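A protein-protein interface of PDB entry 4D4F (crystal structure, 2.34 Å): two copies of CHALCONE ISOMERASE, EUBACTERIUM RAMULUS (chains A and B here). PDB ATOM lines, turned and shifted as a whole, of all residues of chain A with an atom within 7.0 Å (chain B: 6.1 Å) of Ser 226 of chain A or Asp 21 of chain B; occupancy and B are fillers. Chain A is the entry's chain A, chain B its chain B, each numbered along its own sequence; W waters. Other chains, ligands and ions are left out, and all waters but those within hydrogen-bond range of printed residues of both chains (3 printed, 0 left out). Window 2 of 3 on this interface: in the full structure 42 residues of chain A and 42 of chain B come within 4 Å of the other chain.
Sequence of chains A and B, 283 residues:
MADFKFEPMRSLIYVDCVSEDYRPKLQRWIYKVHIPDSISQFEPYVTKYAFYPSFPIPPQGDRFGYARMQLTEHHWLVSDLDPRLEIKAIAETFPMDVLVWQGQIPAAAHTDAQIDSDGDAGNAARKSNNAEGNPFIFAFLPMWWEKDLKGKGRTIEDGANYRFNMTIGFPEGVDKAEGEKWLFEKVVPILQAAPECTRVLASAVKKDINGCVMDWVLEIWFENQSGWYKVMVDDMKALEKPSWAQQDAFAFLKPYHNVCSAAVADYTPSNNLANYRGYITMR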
ATOM      1  N   TYR A 162      31.830 -17.046   5.671  1.00  0.00           N
ATOM      2  CA  TYR A 162      30.572 -17.758   5.636  1.00  0.00           C
ATOM      3  C   TYR A 162      30.351 -17.977   4.162  1.00  0.00           C
ATOM      4  O   TYR A 162      30.002 -17.055   3.449  1.00  0.00           O
ATOM      5  CB  TYR A 162      29.490 -16.884   6.277  1.00  0.00           C
ATOM      6  CG  TYR A 162      28.099 -17.471   6.405  1.00  0.00           C
ATOM      7  CD1 TYR A 162      27.718 -18.191   7.525  1.00  0.00           C
ATOM      8  CD2 TYR A 162      27.145 -17.254   5.423  1.00  0.00           C
ATOM      9  CE1 TYR A 162      26.408 -18.674   7.656  1.00  0.00           C
ATOM     10  CE2 TYR A 162      25.844 -17.723   5.540  1.00  0.00           C
ATOM     11  CZ  TYR A 162      25.473 -18.439   6.642  1.00  0.00           C
ATOM     12  OH  TYR A 162      24.181 -18.918   6.738  1.00  0.00           O
ATOM     13  N   GLU A 196      28.867  -6.203   2.442  1.00  0.00           N
ATOM     14  CA  GLU A 196      28.748  -7.463   3.160  1.00  0.00           C
ATOM     15  C   GLU A 196      29.285  -8.691   2.414  1.00  0.00           C
ATOM     16  O   GLU A 196      29.572  -9.690   3.041  1.00  0.00           O
ATOM     17  CB  GLU A 196      27.290  -7.733   3.529  1.00  0.00           C
ATOM     18  CG  GLU A 196      26.681  -6.675   4.460  1.00  0.00           C
ATOM     19  CD  GLU A 196      26.192  -5.421   3.715  1.00  0.00           C
ATOM     20  OE1 GLU A 196      26.231  -5.342   2.465  1.00  0.00           O
ATOM     21  OE2 GLU A 196      25.771  -4.489   4.396  1.00  0.00           O
ATOM     22  N   PHE A 222      30.251 -14.239   2.752  1.00  0.00           N
ATOM     23  CA  PHE A 222      29.841 -13.212   3.677  1.00  0.00           C
ATOM     24  C   PHE A 222      30.694 -13.361   4.922  1.00  0.00           C
ATOM     25  O   PHE A 222      31.532 -14.257   5.003  1.00  0.00           O
ATOM     26  CB  PHE A 222      28.369 -13.386   4.000  1.00  0.00           C
ATOM     27  CG  PHE A 222      27.502 -13.264   2.793  1.00  0.00           C
ATOM     28  CD1 PHE A 222      27.148 -12.013   2.309  1.00  0.00           C
ATOM     29  CD2 PHE A 222      27.104 -14.381   2.099  1.00  0.00           C
ATOM     30  CE1 PHE A 222      26.386 -11.878   1.172  1.00  0.00           C
ATOM     31  CE2 PHE A 222      26.348 -14.250   0.968  1.00  0.00           C
ATOM     32  CZ  PHE A 222      25.976 -12.997   0.501  1.00  0.00           C
ATOM     33  N   GLU A 223      30.494 -12.470   5.875  1.00  0.00           N
ATOM     34  CA  GLU A 223      31.183 -12.545   7.144  1.00  0.00           C
ATOM     35  C   GLU A 223      30.398 -13.498   8.006  1.00  0.00           C
ATOM     36  O   GLU A 223      30.944 -14.234   8.818  1.00  0.00           O
ATOM     37  CB  GLU A 223      31.222 -11.153   7.787  1.00  0.00           C
ATOM     38  CG  GLU A 223      32.153 -11.056   8.970  1.00  0.00           C
ATOM     39  CD  GLU A 223      32.148  -9.686   9.667  1.00  0.00           C
ATOM     40  OE1 GLU A 223      31.524  -8.732   9.150  1.00  0.00           O
ATOM     41  OE2 GLU A 223      32.772  -9.590  10.749  1.00  0.00           O
ATOM     42  N   ASN A 224      29.089 -13.461   7.828  1.00  0.00           N
ATOM     43  CA  ASN A 224      28.200 -14.200   8.684  1.00  0.00           C
ATOM     44  C   ASN A 224      26.783 -14.236   8.086  1.00  0.00           C
ATOM     45  O   ASN A 224      26.485 -13.597   7.073  1.00  0.00           O
ATOM     46  CB  ASN A 224      28.171 -13.549  10.077  1.00  0.00           C
ATOM     47  CG  ASN A 224      27.888 -12.055  10.016  1.00  0.00           C
ATOM     48  OD1 ASN A 224      27.034 -11.595   9.264  1.00  0.00           O
ATOM     49  ND2 ASN A 224      28.592 -11.290  10.828  1.00  0.00           N
ATOM     50  N   GLN A 225      25.933 -14.969   8.776  1.00  0.00           N
ATOM     51  CA  GLN A 225      24.544 -15.120   8.435  1.00  0.00           C
ATOM     52  C   GLN A 225      23.811 -13.820   8.290  1.00  0.00           C
ATOM     53  O   GLN A 225      23.043 -13.655   7.357  1.00  0.00           O
ATOM     54  CB  GLN A 225      23.888 -15.977   9.523  1.00  0.00           C
ATOM     55  CG  GLN A 225      22.405 -16.213   9.357  1.00  0.00           C
ATOM     56  CD  GLN A 225      21.858 -17.063  10.471  1.00  0.00           C
ATOM     57  OE1 GLN A 225      21.984 -18.298  10.472  1.00  0.00           O
ATOM     58  NE2 GLN A 225      21.250 -16.406  11.441  1.00  0.00           N
ATOM     59  N   SER A 226      23.992 -12.884   9.214  1.00  0.00           N
ATOM     60  CA  SER A 226      23.304 -11.591   9.051  1.00  0.00           C
ATOM     61  C   SER A 226      23.686 -10.958   7.722  1.00  0.00           C
ATOM     62  O   SER A 226      22.857 -10.377   7.050  1.00  0.00           O
ATOM     63  CB  SER A 226      23.619 -10.596  10.172  1.00  0.00           C
ATOM     64  OG  SER A 226      23.272 -11.104  11.423  1.00  0.00           O
ATOM     65  N   GLY A 227      24.944 -11.036   7.352  1.00  0.00           N
ATOM     66  CA  GLY A 227      25.363 -10.474   6.070  1.00  0.00           C
ATOM     67  C   GLY A 227      24.710 -11.194   4.904  1.00  0.00           C
ATOM     68  O   GLY A 227      24.285 -10.564   3.945  1.00  0.00           O
ATOM     69  N   TRP A 228      24.644 -12.518   4.992  1.00  0.00           N
ATOM     70  CA  TRP A 228      24.001 -13.323   3.973  1.00  0.00           C
ATOM     71  C   TRP A 228      22.551 -12.854   3.796  1.00  0.00           C
ATOM     72  O   TRP A 228      22.096 -12.609   2.677  1.00  0.00           O
ATOM     73  CB  TRP A 228      24.062 -14.807   4.347  1.00  0.00           C
ATOM     74  CG  TRP A 228      23.212 -15.649   3.443  1.00  0.00           C
ATOM     75  CD1 TRP A 228      23.598 -16.207   2.280  1.00  0.00           C
ATOM     76  CD2 TRP A 228      21.834 -15.963   3.605  1.00  0.00           C
ATOM     77  NE1 TRP A 228      22.576 -16.887   1.717  1.00  0.00           N
ATOM     78  CE2 TRP A 228      21.461 -16.738   2.494  1.00  0.00           C
ATOM     79  CE3 TRP A 228      20.873 -15.655   4.575  1.00  0.00           C
ATOM     80  CZ2 TRP A 228      20.153 -17.229   2.313  1.00  0.00           C
ATOM     81  CZ3 TRP A 228      19.585 -16.127   4.420  1.00  0.00           C
ATOM     82  CH2 TRP A 228      19.223 -16.909   3.283  1.00  0.00           C
ATOM     83  N   TYR A 229      21.827 -12.718   4.897  1.00  0.00           N
ATOM     84  CA  TYR A 229      20.425 -12.329   4.838  1.00  0.00           C
ATOM     85  C   TYR A 229      20.268 -10.933   4.231  1.00  0.00           C
ATOM     86  O   TYR A 229      19.428 -10.708   3.342  1.00  0.00           O
ATOM     87  CB  TYR A 229      19.795 -12.402   6.239  1.00  0.00           C
ATOM     88  CG  TYR A 229      18.308 -12.147   6.272  1.00  0.00           C
ATOM     89  CD1 TYR A 229      17.815 -10.848   6.360  1.00  0.00           C
ATOM     90  CD2 TYR A 229      17.383 -13.200   6.193  1.00  0.00           C
ATOM     91  CE1 TYR A 229      16.446 -10.602   6.372  1.00  0.00           C
ATOM     92  CE2 TYR A 229      16.022 -12.958   6.214  1.00  0.00           C
ATOM     93  CZ  TYR A 229      15.568 -11.653   6.300  1.00  0.00           C
ATOM     94  OH  TYR A 229      14.234 -11.376   6.294  1.00  0.00           O
ATOM     95  N   LYS A 230      21.111 -10.002   4.665  1.00  0.00           N
ATOM     96  CA  LYS A 230      20.975  -8.633   4.214  1.00  0.00           C
ATOM     97  C   LYS A 230      21.059  -8.570   2.701  1.00  0.00           C
ATOM     98  O   LYS A 230      20.264  -7.904   2.059  1.00  0.00           O
ATOM     99  CB  LYS A 230      22.004  -7.720   4.862  1.00  0.00           C
ATOM    100  CG  LYS A 230      21.883  -6.240   4.480  1.00  0.00           C
ATOM    101  CD  LYS A 230      22.729  -5.922   3.234  1.00  0.00           C
ATOM    102  CE  LYS A 230      22.905  -4.413   2.959  1.00  0.00           C
ATOM    103  NZ  LYS A 230      23.790  -4.164   1.754  1.00  0.00           N
ATOM    104  N   VAL A 231      21.997  -9.274   2.117  1.00  0.00           N
ATOM    105  CA  VAL A 231      22.195  -9.214   0.674  1.00  0.00           C
ATOM    106  C   VAL A 231      21.220 -10.131  -0.110  1.00  0.00           C
ATOM    107  O   VAL A 231      20.549  -9.670  -1.061  1.00  0.00           O
ATOM    108  CB  VAL A 231      23.647  -9.587   0.345  1.00  0.00           C
ATOM    109  CG1 VAL A 231      23.862  -9.643  -1.143  1.00  0.00           C
ATOM    110  CG2 VAL A 231      24.597  -8.586   0.983  1.00  0.00           C
ATOM    111  N   SER B  19      25.727 -16.800  19.424  1.00  0.00           N
ATOM    112  CA  SER B  19      25.056 -16.186  18.313  1.00  0.00           C
ATOM    113  C   SER B  19      25.566 -16.815  17.026  1.00  0.00           C
ATOM    114  O   SER B  19      26.753 -17.090  16.914  1.00  0.00           O
ATOM    115  CB  SER B  19      25.352 -14.694  18.350  1.00  0.00           C
ATOM    116  OG  SER B  19      25.128 -14.169  17.078  1.00  0.00           O
ATOM    117  N   GLU B  20      24.682 -17.045  16.057  1.00  0.00           N
ATOM    118  CA  GLU B  20      25.114 -17.604  14.776  1.00  0.00           C
ATOM    119  C   GLU B  20      26.128 -16.742  14.073  1.00  0.00           C
ATOM    120  O   GLU B  20      26.983 -17.258  13.337  1.00  0.00           O
ATOM    121  CB  GLU B  20      23.928 -17.878  13.840  1.00  0.00           C
ATOM    122  CG  GLU B  20      23.116 -19.102  14.254  1.00  0.00           C
ATOM    123  CD  GLU B  20      23.992 -20.314  14.547  1.00  0.00           C
ATOM    124  OE1 GLU B  20      24.806 -20.644  13.644  1.00  0.00           O
ATOM    125  OE2 GLU B  20      23.909 -20.896  15.690  1.00  0.00           O
ATOM    126  N   ASP B  21      26.060 -15.435  14.276  1.00  0.00           N
ATOM    127  CA  ASP B  21      27.040 -14.544  13.627  1.00  0.00           C
ATOM    128  C   ASP B  21      28.460 -14.775  14.102  1.00  0.00           C
ATOM    129  O   ASP B  21      29.418 -14.433  13.390  1.00  0.00           O
ATOM    130  CB  ASP B  21      26.648 -13.062  13.789  1.00  0.00           C
ATOM    131  CG  ASP B  21      25.550 -12.648  12.786  1.00  0.00           C
ATOM    132  OD1 ASP B  21      25.286 -13.418  11.798  1.00  0.00           O
ATOM    133  OD2 ASP B  21      24.968 -11.555  12.970  1.00  0.00           O
ATOM    134  N   TYR B  22      28.593 -15.349  15.291  1.00  0.00           N
ATOM    135  CA  TYR B  22      29.900 -15.709  15.819  1.00  0.00           C
ATOM    136  C   TYR B  22      30.423 -17.078  15.363  1.00  0.00           C
ATOM    137  O   TYR B  22      31.618 -17.372  15.562  1.00  0.00           O
ATOM    138  CB  TYR B  22      29.899 -15.719  17.358  1.00  0.00           C
ATOM    139  CG  TYR B  22      29.540 -14.423  18.064  1.00  0.00           C
ATOM    140  CD1 TYR B  22      29.870 -13.176  17.537  1.00  0.00           C
ATOM    141  CD2 TYR B  22      28.923 -14.462  19.316  1.00  0.00           C
ATOM    142  CE1 TYR B  22      29.567 -12.006  18.235  1.00  0.00           C
ATOM    143  CE2 TYR B  22      28.609 -13.312  20.005  1.00  0.00           C
ATOM    144  CZ  TYR B  22      28.938 -12.092  19.464  1.00  0.00           C
ATOM    145  OH  TYR B  22      28.622 -10.976  20.182  1.00  0.00           O
ATOM    146  N   ARG B  23      29.568 -17.922  14.791  1.00  0.00           N
ATOM    147  CA  ARG B  23      29.979 -19.303  14.473  1.00  0.00           C
ATOM    148  C   ARG B  23      31.221 -19.381  13.588  1.00  0.00           C
ATOM    149  O   ARG B  23      32.155 -20.091  13.893  1.00  0.00           O
ATOM    150  CB  ARG B  23      28.838 -20.122  13.858  1.00  0.00           C
ATOM    151  CG  ARG B  23      29.125 -21.622  13.763  1.00  0.00           C
ATOM    152  CD  ARG B  23      27.893 -22.373  13.266  1.00  0.00           C
ATOM    153  NE  ARG B  23      26.852 -22.351  14.283  1.00  0.00           N
ATOM    154  CZ  ARG B  23      26.829 -23.174  15.318  1.00  0.00           C
ATOM    155  NH1 ARG B  23      27.758 -24.089  15.459  1.00  0.00           N
ATOM    156  NH2 ARG B  23      25.888 -23.071  16.230  1.00  0.00           N
ATOM    157  N   PRO B  24      31.243 -18.657  12.491  1.00  0.00           N
ATOM    158  CA  PRO B  24      32.428 -18.787  11.650  1.00  0.00           C
ATOM    159  C   PRO B  24      33.741 -18.405  12.372  1.00  0.00           C
ATOM    160  O   PRO B  24      34.775 -19.053  12.183  1.00  0.00           O
ATOM    161  CB  PRO B  24      32.140 -17.836  10.496  1.00  0.00           C
ATOM    162  CG  PRO B  24      30.655 -17.719  10.472  1.00  0.00           C
ATOM    163  CD  PRO B  24      30.263 -17.739  11.911  1.00  0.00           C
ATOM    164  N   LYS B  25      33.680 -17.393  13.216  1.00  0.00           N
ATOM    165  CA  LYS B  25      34.886 -16.918  13.884  1.00  0.00           C
ATOM    166  C   LYS B  25      35.301 -17.885  14.959  1.00  0.00           C
ATOM    167  O   LYS B  25      36.481 -18.220  15.074  1.00  0.00           O
ATOM    168  CB  LYS B  25      34.672 -15.536  14.491  1.00  0.00           C
ATOM    169  CG  LYS B  25      34.782 -14.397  13.504  1.00  0.00           C
ATOM    170  CD  LYS B  25      34.389 -13.085  14.179  1.00  0.00           C
ATOM    171  CE  LYS B  25      34.467 -11.935  13.191  1.00  0.00           C
ATOM    172  NZ  LYS B  25      33.393 -12.033  12.120  1.00  0.00           N
HETATM  173  O   HOH W   1      30.821 -12.273  12.700  1.00  0.00           O
HETATM  174  O   HOH W   2      27.081 -16.910  10.693  1.00  0.00           O
HETATM  175  O   HOH W   3      33.207 -14.172  10.122  1.00  0.00           O
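The side-chain carboxylate (OE2) of Glu 223 of chain A lies within salt-bridge range of the side-chain amino group (NZ) of Lys 25 of chain B, at 2.9 Å.
OD1 of Asp 21 of chain B lies within hydrogen-bond range of N of Gln 225 of chain A (3.5 Å).
The side-chain carboxylate (OD1) of Asp 21 of chain B sits at hydrogen-bond distance from the backbone NH (N) of Ser 226 of chain A, at 2.9 Å.
N of Ser 226 of chain A sits close to OD1 of Asn 224 of chain A (3.3 Å).
The side-chain amide oxygen of Asn 224 of chain A sits at hydrogen-bond distance from the backbone NH of Gly 227 of chain A.
The backbone NH of Asp 21 of chain B lies close to the side-chain hydroxyl of Ser 19 of chain B, at 3.2 Å.
The guanidinium group (NE) of Arg 23 of chain B is in salt-bridge range of the side-chain carboxylate (OE1) of Glu 20 of chain B (2.7 Å).
O of Glu 223 of chain A touches CG of Pro 24 of chain B, 3.9 Å away.
Asn 224 of chain A touches Asp 21 of chain B.
Gln 225 of chain A touches Glu 20 of chain B.
Of chain B, only Asp 21 (2.3 Å) comes within 4 Å of Ser 226 of chain A.
Of chain A, only Asn 224 (3.4 Å), Gln 225 (3.5 Å) and Ser 226 (2.3 Å) come within 4 Å of Asp 21 of chain B.
Of the printed residues of chain B, Glu 223 of chain A touches Pro 24 and Lys 25.
Printed residues of chain A within 4 Å of Lys 25 of chain B: Glu 223.
Printed residues of chain A within 4 Å of Pro 24 of chain B: Glu 223 (3.9 Å).
Tyr 162 of chain A touches none of the printed residues of chain B.
Ser 19 of chain B touches none of the printed residues of chain A.
The nearest printed residue of chain B that does not touch Gln 225 of chain A is Pro 24 of chain B (5.7 Å).
Printed residues of chain A that touch a printed residue of chain B: Glu 223, Asn 224, Gln 225 and Ser 226.
Hydrophobic or aromatic side chains of chain B within 4 Å of the printed part of chain A: Pro 24.
Among the printed residues, 6 pairs touch across the chains.
No position is printed for both chains.
Water W3 lies within hydrogen-bond range of the backbone carbonyl oxygen of Glu 223 of chain A and the side-chain amino group of Lys 25 of chain B.
Water W1 lies within hydrogen-bond range of NZ of Lys 25 of chain B (2.6 Å), O of Asp 21 of chain B (2.7 Å) and ND2 of Asn 224 of chain A (3.1 Å).
Water W2 bridges the backbone carbonyl oxygen of Glu 20 of chain B (2.7 Å) and the backbone NH of Gln 225 of chain A (3.0 Å).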
